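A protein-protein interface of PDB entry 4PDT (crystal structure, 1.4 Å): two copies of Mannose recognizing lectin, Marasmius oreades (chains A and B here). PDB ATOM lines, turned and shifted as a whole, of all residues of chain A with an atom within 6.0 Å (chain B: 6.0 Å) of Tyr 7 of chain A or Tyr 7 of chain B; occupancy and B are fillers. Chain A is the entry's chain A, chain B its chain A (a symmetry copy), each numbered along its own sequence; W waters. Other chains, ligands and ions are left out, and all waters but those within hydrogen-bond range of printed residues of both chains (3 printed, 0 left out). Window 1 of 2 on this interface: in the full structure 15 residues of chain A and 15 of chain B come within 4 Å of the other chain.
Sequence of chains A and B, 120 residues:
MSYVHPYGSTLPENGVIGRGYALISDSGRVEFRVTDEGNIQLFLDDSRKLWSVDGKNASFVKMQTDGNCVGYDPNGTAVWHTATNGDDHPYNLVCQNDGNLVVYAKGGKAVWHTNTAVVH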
ATOM      1  N   HIS A   5       0.987  -1.654 -24.496  1.00  0.00           N
ATOM      2  CA  HIS A   5       0.868  -2.081 -25.893  1.00  0.00           C
ATOM      3  C   HIS A   5       1.925  -1.346 -26.764  1.00  0.00           C
ATOM      4  O   HIS A   5       1.680  -0.242 -27.245  1.00  0.00           O
ATOM      5  CB  HIS A   5      -0.548  -1.774 -26.390  1.00  0.00           C
ATOM      6  CG  HIS A   5      -1.619  -2.470 -25.607  1.00  0.00           C
ATOM      7  ND1 HIS A   5      -2.702  -1.806 -25.118  1.00  0.00           N
ATOM      8  CD2 HIS A   5      -1.704  -3.728 -25.117  1.00  0.00           C
ATOM      9  CE1 HIS A   5      -3.437  -2.620 -24.389  1.00  0.00           C
ATOM     10  NE2 HIS A   5      -2.889  -3.816 -24.430  1.00  0.00           N
ATOM     11  N   PRO A   6       3.105  -1.965 -26.935  1.00  0.00           N
ATOM     12  CA  PRO A   6       4.153  -1.245 -27.724  1.00  0.00           C
ATOM     13  C   PRO A   6       4.094  -1.464 -29.213  1.00  0.00           C
ATOM     14  O   PRO A   6       4.845  -0.877 -29.978  1.00  0.00           O
ATOM     15  CB  PRO A   6       5.449  -1.878 -27.232  1.00  0.00           C
ATOM     16  CG  PRO A   6       5.114  -2.786 -26.085  1.00  0.00           C
ATOM     17  CD  PRO A   6       3.654  -3.127 -26.221  1.00  0.00           C
ATOM     18  N   TYR A   7       3.135  -2.305 -29.643  1.00  0.00           N
ATOM     19  CA  TYR A   7       3.052  -2.772 -31.036  1.00  0.00           C
ATOM     20  C   TYR A   7       1.670  -2.757 -31.664  1.00  0.00           C
ATOM     21  O   TYR A   7       1.533  -3.310 -32.771  1.00  0.00           O
ATOM     22  CB  TYR A   7       3.516  -4.223 -31.097  1.00  0.00           C
ATOM     23  CG  TYR A   7       5.004  -4.425 -30.815  1.00  0.00           C
ATOM     24  CD1 TYR A   7       5.944  -4.165 -31.805  1.00  0.00           C
ATOM     25  CD2 TYR A   7       5.436  -4.985 -29.629  1.00  0.00           C
ATOM     26  CE1 TYR A   7       7.292  -4.433 -31.598  1.00  0.00           C
ATOM     27  CE2 TYR A   7       6.798  -5.224 -29.381  1.00  0.00           C
ATOM     28  CZ  TYR A   7       7.719  -4.957 -30.394  1.00  0.00           C
ATOM     29  OH  TYR A   7       9.034  -5.255 -30.117  1.00  0.00           O
ATOM     30  N   GLY A   8       0.686  -2.157 -31.020  1.00  0.00           N
ATOM     31  CA  GLY A   8      -0.698  -2.254 -31.534  1.00  0.00           C
ATOM     32  C   GLY A   8      -1.097  -3.717 -31.506  1.00  0.00           C
ATOM     33  O   GLY A   8      -0.941  -4.424 -30.527  1.00  0.00           O
ATOM     34  N   SER A   9      -1.641  -4.141 -32.651  1.00  0.00           N
ATOM     35  CA  SER A   9      -2.102  -5.517 -32.780  1.00  0.00           C
ATOM     36  C   SER A   9      -1.071  -6.545 -33.260  1.00  0.00           C
ATOM     37  O   SER A   9      -1.330  -7.726 -33.288  1.00  0.00           O
ATOM     38  CB  SER A   9      -3.206  -5.572 -33.887  1.00  0.00           C
ATOM     39  OG  SER A   9      -2.636  -5.338 -35.160  1.00  0.00           O
ATOM     40  N   THR A  10       0.109  -6.108 -33.675  1.00  0.00           N
ATOM     41  CA  THR A  10       0.974  -6.965 -34.477  1.00  0.00           C
ATOM     42  C   THR A  10       2.409  -7.003 -34.037  1.00  0.00           C
ATOM     43  O   THR A  10       3.042  -5.919 -33.885  1.00  0.00           O
ATOM     44  CB  THR A  10       0.918  -6.481 -35.931  1.00  0.00           C
ATOM     45  OG1 THR A  10      -0.469  -6.574 -36.409  1.00  0.00           O
ATOM     46  CG2 THR A  10       1.809  -7.279 -36.828  1.00  0.00           C
ATOM     47  N   LEU A  11       2.928  -8.186 -33.851  1.00  0.00           N
ATOM     48  CA  LEU A  11       4.318  -8.383 -33.456  1.00  0.00           C
ATOM     49  C   LEU A  11       5.118  -8.667 -34.723  1.00  0.00           C
ATOM     50  O   LEU A  11       4.994  -9.719 -35.346  1.00  0.00           O
ATOM     51  CB  LEU A  11       4.444  -9.508 -32.471  1.00  0.00           C
ATOM     52  CG  LEU A  11       5.736  -9.553 -31.664  1.00  0.00           C
ATOM     53  CD1 LEU A  11       5.885  -8.311 -30.783  1.00  0.00           C
ATOM     54  CD2 LEU A  11       5.756 -10.843 -30.854  1.00  0.00           C
ATOM     55  N   PRO A  12       5.923  -7.678 -35.167  1.00  0.00           N
ATOM     56  CA  PRO A  12       6.705  -7.883 -36.356  1.00  0.00           C
ATOM     57  C   PRO A  12       7.993  -8.663 -36.049  1.00  0.00           C
ATOM     58  O   PRO A  12       8.328  -8.973 -34.903  1.00  0.00           O
ATOM     59  CB  PRO A  12       7.064  -6.438 -36.791  1.00  0.00           C
ATOM     60  CG  PRO A  12       7.135  -5.750 -35.499  1.00  0.00           C
ATOM     61  CD  PRO A  12       6.177  -6.361 -34.547  1.00  0.00           C
ATOM     62  N   ASN A  14      11.518  -9.495 -35.095  1.00  0.00           N
ATOM     63  CA  ASN A  14      12.350  -8.976 -34.002  1.00  0.00           C
ATOM     64  C   ASN A  14      11.547  -8.409 -32.876  1.00  0.00           C
ATOM     65  O   ASN A  14      12.115  -7.945 -31.898  1.00  0.00           O
ATOM     66  CB  ASN A  14      13.430  -7.974 -34.467  1.00  0.00           C
ATOM     67  CG  ASN A  14      14.588  -8.678 -35.133  1.00  0.00           C
ATOM     68  OD1 ASN A  14      15.035  -9.738 -34.673  1.00  0.00           O
ATOM     69  ND2 ASN A  14      15.088  -8.103 -36.191  1.00  0.00           N
ATOM     70  N   GLY A  15      10.220  -8.424 -32.960  1.00  0.00           N
ATOM     71  CA  GLY A  15       9.368  -7.934 -31.913  1.00  0.00           C
ATOM     72  C   GLY A  15       9.302  -8.875 -30.724  1.00  0.00           C
ATOM     73  O   GLY A  15       9.360 -10.094 -30.881  1.00  0.00           O
ATOM     74  N   VAL A  16       9.289  -8.286 -29.529  1.00  0.00           N
ATOM     75  CA  VAL A  16       9.210  -9.024 -28.296  1.00  0.00           C
ATOM     76  C   VAL A  16       8.178  -8.387 -27.377  1.00  0.00           C
ATOM     77  O   VAL A  16       8.184  -7.151 -27.194  1.00  0.00           O
ATOM     78  CB  VAL A  16      10.607  -9.041 -27.559  1.00  0.00           C
ATOM     79  CG1 VAL A  16      10.438  -9.522 -26.123  1.00  0.00           C
ATOM     80  CG2 VAL A  16      11.595  -9.890 -28.352  1.00  0.00           C
ATOM     81  N   ILE A  17       7.314  -9.210 -26.764  1.00  0.00           N
ATOM     82  CA  ILE A  17       6.497  -8.727 -25.665  1.00  0.00           C
ATOM     83  C   ILE A  17       6.904  -9.491 -24.384  1.00  0.00           C
ATOM     84  O   ILE A  17       7.005 -10.713 -24.359  1.00  0.00           O
ATOM     85  CB  ILE A  17       4.967  -8.707 -25.855  1.00  0.00           C
ATOM     86  CG1 ILE A  17       4.507 -10.017 -26.409  1.00  0.00           C
ATOM     87  CG2 ILE A  17       4.554  -7.508 -26.731  1.00  0.00           C
ATOM     88  CD1 ILE A  17       2.981 -10.213 -26.456  1.00  0.00           C
ATOM     89  N   ALA A  22       1.548  -6.594 -24.088  1.00  0.00           N
ATOM     90  CA  ALA A  22       0.529  -7.340 -24.874  1.00  0.00           C
ATOM     91  C   ALA A  22       0.354  -6.756 -26.255  1.00  0.00           C
ATOM     92  O   ALA A  22       0.598  -5.564 -26.480  1.00  0.00           O
ATOM     93  CB  ALA A  22      -0.858  -7.380 -24.141  1.00  0.00           C
ATOM     94  N   LEU A  23      -0.191  -7.587 -27.158  1.00  0.00           N
ATOM     95  CA  LEU A  23      -0.792  -7.097 -28.388  1.00  0.00           C
ATOM     96  C   LEU A  23      -2.267  -6.808 -28.081  1.00  0.00           C
ATOM     97  O   LEU A  23      -2.865  -7.518 -27.246  1.00  0.00           O
ATOM     98  CB  LEU A  23      -0.666  -8.071 -29.512  1.00  0.00           C
ATOM     99  CG  LEU A  23       0.696  -8.633 -29.889  1.00  0.00           C
ATOM    100  CD1 LEU A  23       0.591  -9.711 -30.964  1.00  0.00           C
ATOM    101  CD2 LEU A  23       1.591  -7.432 -30.272  1.00  0.00           C
ATOM    102  N   LYS A  62       8.825 -13.806 -28.732  1.00  0.00           N
ATOM    103  CA  LYS A  62       9.551 -13.159 -29.803  1.00  0.00           C
ATOM    104  C   LYS A  62       9.130 -13.673 -31.186  1.00  0.00           C
ATOM    105  O   LYS A  62       9.178 -14.894 -31.416  1.00  0.00           O
ATOM    106  CB  LYS A  62      11.054 -13.421 -29.572  1.00  0.00           C
ATOM    107  CG  LYS A  62      11.969 -12.619 -30.513  1.00  0.00           C
ATOM    108  CD  LYS A  62      13.411 -12.626 -30.061  1.00  0.00           C
ATOM    109  CE  LYS A  62      14.250 -11.598 -30.823  1.00  0.00           C
ATOM    110  NZ  LYS A  62      15.704 -11.643 -30.458  1.00  0.00           N
ATOM    111  N   HIS B   5      17.212 -10.837 -20.854  1.00  0.00           N
ATOM    112  CA  HIS B   5      17.932 -10.372 -22.043  1.00  0.00           C
ATOM    113  C   HIS B   5      17.373 -11.076 -23.310  1.00  0.00           C
ATOM    114  O   HIS B   5      17.813 -12.169 -23.664  1.00  0.00           O
ATOM    115  CB  HIS B   5      19.425 -10.676 -21.871  1.00  0.00           C
ATOM    116  CG  HIS B   5      20.036 -10.007 -20.677  1.00  0.00           C
ATOM    117  ND1 HIS B   5      20.796 -10.691 -19.779  1.00  0.00           N
ATOM    118  CD2 HIS B   5      19.888  -8.764 -20.166  1.00  0.00           C
ATOM    119  CE1 HIS B   5      21.129  -9.903 -18.779  1.00  0.00           C
ATOM    120  NE2 HIS B   5      20.647  -8.702 -19.024  1.00  0.00           N
ATOM    121  N   PRO B   6      16.386 -10.446 -23.968  1.00  0.00           N
ATOM    122  CA  PRO B   6      15.798 -11.137 -25.158  1.00  0.00           C
ATOM    123  C   PRO B   6      16.507 -10.877 -26.461  1.00  0.00           C
ATOM    124  O   PRO B   6      16.174 -11.438 -27.494  1.00  0.00           O
ATOM    125  CB  PRO B   6      14.415 -10.509 -25.270  1.00  0.00           C
ATOM    126  CG  PRO B   6      14.203  -9.635 -24.069  1.00  0.00           C
ATOM    127  CD  PRO B   6      15.571  -9.300 -23.537  1.00  0.00           C
ATOM    128  N   TYR B   7      17.552 -10.031 -26.400  1.00  0.00           N
ATOM    129  CA  TYR B   7      18.239  -9.527 -27.600  1.00  0.00           C
ATOM    130  C   TYR B   7      19.756  -9.532 -27.554  1.00  0.00           C
ATOM    131  O   TYR B   7      20.364  -8.951 -28.471  1.00  0.00           O
ATOM    132  CB  TYR B   7      17.840  -8.072 -27.820  1.00  0.00           C
ATOM    133  CG  TYR B   7      16.379  -7.868 -28.218  1.00  0.00           C
ATOM    134  CD1 TYR B   7      15.974  -8.094 -29.528  1.00  0.00           C
ATOM    135  CD2 TYR B   7      15.464  -7.338 -27.330  1.00  0.00           C
ATOM    136  CE1 TYR B   7      14.671  -7.824 -29.930  1.00  0.00           C
ATOM    137  CE2 TYR B   7      14.132  -7.097 -27.702  1.00  0.00           C
ATOM    138  CZ  TYR B   7      13.754  -7.330 -29.024  1.00  0.00           C
ATOM    139  OH  TYR B   7      12.449  -7.032 -29.348  1.00  0.00           O
ATOM    140  N   GLY B   8      20.359 -10.157 -26.558  1.00  0.00           N
ATOM    141  CA  GLY B   8      21.827 -10.055 -26.406  1.00  0.00           C
ATOM    142  C   GLY B   8      22.163  -8.595 -26.164  1.00  0.00           C
ATOM    143  O   GLY B   8      21.586  -7.915 -25.335  1.00  0.00           O
ATOM    144  N   SER B   9      23.154  -8.143 -26.939  1.00  0.00           N
ATOM    145  CA  SER B   9      23.615  -6.768 -26.814  1.00  0.00           C
ATOM    146  C   SER B   9      22.896  -5.721 -27.672  1.00  0.00           C
ATOM    147  O   SER B   9      23.133  -4.541 -27.550  1.00  0.00           O
ATOM    148  CB  SER B   9      25.094  -6.689 -27.318  1.00  0.00           C
ATOM    149  OG  SER B   9      25.146  -6.884 -28.718  1.00  0.00           O
ATOM    150  N   THR B  10      22.023  -6.137 -28.577  1.00  0.00           N
ATOM    151  CA  THR B  10      21.595  -5.254 -29.654  1.00  0.00           C
ATOM    152  C   THR B  10      20.113  -5.219 -29.892  1.00  0.00           C
ATOM    153  O   THR B  10      19.484  -6.303 -30.065  1.00  0.00           O
ATOM    154  CB  THR B  10      22.291  -5.698 -30.948  1.00  0.00           C
ATOM    155  OG1 THR B  10      23.745  -5.601 -30.760  1.00  0.00           O
ATOM    156  CG2 THR B  10      21.881  -4.870 -32.123  1.00  0.00           C
ATOM    157  N   LEU B  11      19.558  -4.038 -29.922  1.00  0.00           N
ATOM    158  CA  LEU B  11      18.135  -3.843 -30.175  1.00  0.00           C
ATOM    159  C   LEU B  11      17.974  -3.519 -31.657  1.00  0.00           C
ATOM    160  O   LEU B  11      18.353  -2.451 -32.132  1.00  0.00           O
ATOM    161  CB  LEU B  11      17.580  -2.745 -29.317  1.00  0.00           C
ATOM    162  CG  LEU B  11      16.064  -2.713 -29.162  1.00  0.00           C
ATOM    163  CD1 LEU B  11      15.549  -3.978 -28.472  1.00  0.00           C
ATOM    164  CD2 LEU B  11      15.680  -1.446 -28.409  1.00  0.00           C
ATOM    165  N   PRO B  12      17.455  -4.490 -32.437  1.00  0.00           N
ATOM    166  CA  PRO B  12      17.277  -4.248 -33.844  1.00  0.00           C
ATOM    167  C   PRO B  12      15.980  -3.468 -34.115  1.00  0.00           C
ATOM    168  O   PRO B  12      15.172  -3.188 -33.226  1.00  0.00           O
ATOM    169  CB  PRO B  12      17.155  -5.678 -34.433  1.00  0.00           C
ATOM    170  CG  PRO B  12      16.526  -6.402 -33.323  1.00  0.00           C
ATOM    171  CD  PRO B  12      16.962  -5.823 -32.030  1.00  0.00           C
ATOM    172  N   ASN B  14      12.391  -2.641 -34.793  1.00  0.00           N
ATOM    173  CA  ASN B  14      11.165  -3.184 -34.194  1.00  0.00           C
ATOM    174  C   ASN B  14      11.392  -3.786 -32.845  1.00  0.00           C
ATOM    175  O   ASN B  14      10.455  -4.274 -32.231  1.00  0.00           O
ATOM    176  CB  ASN B  14      10.407  -4.166 -35.116  1.00  0.00           C
ATOM    177  CG  ASN B  14       9.658  -3.436 -36.204  1.00  0.00           C
ATOM    178  OD1 ASN B  14       9.048  -2.387 -35.961  1.00  0.00           O
ATOM    179  ND2 ASN B  14       9.680  -3.979 -37.389  1.00  0.00           N
ATOM    180  N   GLY B  15      12.620  -3.778 -32.335  1.00  0.00           N
ATOM    181  CA  GLY B  15      12.925  -4.302 -31.033  1.00  0.00           C
ATOM    182  C   GLY B  15      12.454  -3.395 -29.911  1.00  0.00           C
ATOM    183  O   GLY B  15      12.463  -2.171 -30.044  1.00  0.00           O
ATOM    184  N   VAL B  16      11.941  -4.016 -28.850  1.00  0.00           N
ATOM    185  CA  VAL B  16      11.463  -3.313 -27.689  1.00  0.00           C
ATOM    186  C   VAL B  16      11.988  -3.981 -26.427  1.00  0.00           C
ATOM    187  O   VAL B  16      11.910  -5.222 -26.299  1.00  0.00           O
ATOM    188  CB  VAL B  16       9.885  -3.308 -27.644  1.00  0.00           C
ATOM    189  CG1 VAL B  16       9.400  -2.867 -26.268  1.00  0.00           C
ATOM    190  CG2 VAL B  16       9.343  -2.431 -28.768  1.00  0.00           C
ATOM    191  N   ILE B  17      12.487  -3.180 -25.474  1.00  0.00           N
ATOM    192  CA  ILE B  17      12.738  -3.699 -24.140  1.00  0.00           C
ATOM    193  C   ILE B  17      11.803  -2.968 -23.150  1.00  0.00           C
ATOM    194  O   ILE B  17      11.694  -1.747 -23.138  1.00  0.00           O
ATOM    195  CB  ILE B  17      14.195  -3.724 -23.635  1.00  0.00           C
ATOM    196  CG1 ILE B  17      14.845  -2.402 -23.893  1.00  0.00           C
ATOM    197  CG2 ILE B  17      14.960  -4.901 -24.272  1.00  0.00           C
ATOM    198  CD1 ILE B  17      16.233  -2.214 -23.256  1.00  0.00           C
ATOM    199  N   ALA B  22      16.498  -5.906 -20.600  1.00  0.00           N
ATOM    200  CA  ALA B  22      17.754  -5.146 -20.834  1.00  0.00           C
ATOM    201  C   ALA B  22      18.523  -5.692 -22.011  1.00  0.00           C
ATOM    202  O   ALA B  22      18.412  -6.876 -22.354  1.00  0.00           O
ATOM    203  CB  ALA B  22      18.675  -5.135 -19.563  1.00  0.00           C
ATOM    204  N   LEU B  23      19.406  -4.840 -22.558  1.00  0.00           N
ATOM    205  CA  LEU B  23      20.491  -5.300 -23.410  1.00  0.00           C
ATOM    206  C   LEU B  23      21.681  -5.607 -22.491  1.00  0.00           C
ATOM    207  O   LEU B  23      21.845  -4.924 -21.459  1.00  0.00           O
ATOM    208  CB  LEU B  23      20.868  -4.296 -24.447  1.00  0.00           C
ATOM    209  CG  LEU B  23      19.808  -3.714 -25.370  1.00  0.00           C
ATOM    210  CD1 LEU B  23      20.371  -2.608 -26.258  1.00  0.00           C
ATOM    211  CD2 LEU B  23      19.183  -4.899 -26.143  1.00  0.00           C
ATOM    212  N   LYS B  62      11.972   1.477 -27.778  1.00  0.00           N
ATOM    213  CA  LYS B  62      11.797   0.864 -29.078  1.00  0.00           C
ATOM    214  C   LYS B  62      12.781   1.413 -30.118  1.00  0.00           C
ATOM    215  O   LYS B  62      12.832   2.641 -30.312  1.00  0.00           O
ATOM    216  CB  LYS B  62      10.344   1.129 -29.526  1.00  0.00           C
ATOM    217  CG  LYS B  62       9.943   0.359 -30.796  1.00  0.00           C
ATOM    218  CD  LYS B  62       8.450   0.363 -31.027  1.00  0.00           C
ATOM    219  CE  LYS B  62       8.040  -0.637 -32.109  1.00  0.00           C
ATOM    220  NZ  LYS B  62       6.574  -0.594 -32.423  1.00  0.00           N
HETATM  221  O   HOH W   1      18.359 -12.710 -29.417  1.00  0.00           O
HETATM  222  O   HOH W   2       3.725   0.461 -32.631  1.00  0.00           O
HETATM  223  O   HOH W   3       9.687  -6.209 -25.198  1.00  0.00           O
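The side-chain hydroxyl (OH) of Tyr 7 of chain A lies close to the backbone NH (N) of Val 16 of chain B, 3.4 Å away. The backbone carbonyl oxygen (O) of Asn 14 of chain B sits at hydrogen-bond distance from the side-chain hydroxyl (OH) of Tyr 7 of chain A (2.7 Å). O of Pro 6 of chain A is in hydrogen-bond range of NZ of Lys 62 of chain B. The backbone carbonyl oxygen (O) of Asn 14 of chain A is in hydrogen-bond range of the side-chain hydroxyl (OH) of Tyr 7 of chain B (2.7 Å). OH of Tyr 7 of chain B lies close to N of Val 16 of chain A. The side-chain amino group (NZ) of Lys 62 of chain A lies within hydrogen-bond range of the backbone carbonyl oxygen (O) of Pro 6 of chain B.
The side-chain hydroxyl (OH) of Tyr 7 of chain B sits at hydrogen-bond distance from the backbone NH (N) of Val 16 of chain B, 3.1 Å away. The side-chain hydroxyl (OH) of Tyr 7 of chain A sits at hydrogen-bond distance from the backbone NH (N) of Val 16 of chain A.
Among the printed residues, merely in contact across the chains: Tyr 7 of chain A with Tyr 7 of chain B, Tyr 7 of chain A with Gly 15 of chain B, Tyr 7 of chain A with Lys 62 of chain B, Pro 12 of chain A with Asn 14 of chain B, Asn 14 of chain A with Pro 12 of chain B, Asn 14 of chain A with Gly 15 of chain B, Gly 15 of chain A with Tyr 7 of chain B, Gly 15 of chain A with Asn 14 of chain B and Lys 62 of chain A with Tyr 7 of chain B.
Of chain B, only Tyr 7 (3.9 Å), Asn 14 (2.7 Å), Gly 15 (3.9 Å), Val 16 (3.1 Å) and Lys 62 (3.7 Å) come within 4 Å of Tyr 7 of chain A. Tyr 7 of chain B touches five residues of chain A. Of the printed residues of chain A, Pro 6 of chain B touches Lys 62. Printed residues of chain A within 4 Å of Asn 14 of chain B: Tyr 7, Pro 12 and Gly 15. Of the printed residues of chain A, Val 16 of chain B touches Tyr 7. Printed residues of chain A within 4 Å of Gly 15 of chain B: Tyr 7 (3.9 Å) and Asn 14 (3.8 Å). Of the printed residues of chain B, Asn 14 of chain A touches Tyr 7 (2.7 Å), Pro 12 (3.5 Å) and Gly 15 (3.8 Å). Leu 11 of chain A touches none of the printed residues of chain B. Ala 22 of chain B touches none of the printed residues of chain A. The nearest printed residue of chain B that does not touch Tyr 7 of chain A is Ile 17 of chain B (6.1 Å). The nearest printed residue of chain A that does not touch Tyr 7 of chain B is Ile 17 of chain A (6.1 Å).
Of the 15 printed residues of chain A, 7 touch a printed residue of chain B. Printed residues of chain A that touch a printed residue of chain B: Pro 6, Tyr 7, Pro 12, Asn 14, Gly 15, Val 16 and Lys 62. Printed residues of chain B that touch a printed residue of chain A: Pro 6, Tyr 7, Pro 12, Asn 14, Gly 15, Val 16 and Lys 62. Hydrophobic or aromatic side chains of chain B that line the printed part of chain A: Tyr 7, Pro 12 and Val 16. Among the printed residues, 15 pairs touch across the chains. Among the printed residues, no Asp or Glu carboxylate lies within 4 Å of a Lys or Arg side-chain nitrogen of the other chain.
Tyr 7 of chain A touches its own counterpart, Tyr 7 of chain B. Tyr 7 of chain A touches Val 16 of chain B, and with the chains exchanged Val 16 of chain A touches Tyr 7 of chain B. Pro 12 of chain A touches Asn 14 of chain B, and with the chains exchanged Asn 14 of chain A touches Pro 12 of chain B. Asn 14 of chain A touches Gly 15 of chain B, and with the chains exchanged Gly 15 of chain A touches Asn 14 of chain B. 15 positions are printed for both chains. Of the 15 pairs that touch across the chains among the printed residues, 15 have their exchanged pair printed and touching as well.
Water W3 lies within hydrogen-bond range of O of Val 16 of chain B (2.7 Å) and O of Val 16 of chain A (2.7 Å). Water W2 bridges the side-chain amino group (NZ) of Lys 62 of chain B (3.0 Å) and the backbone carbonyl oxygen (O) of Pro 6 of chain A (3.2 Å). Water W1 bridges the side-chain amino group (NZ) of Lys 62 of chain A (3.0 Å) and the backbone carbonyl oxygen (O) of Pro 6 of chain B (3.2 Å).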
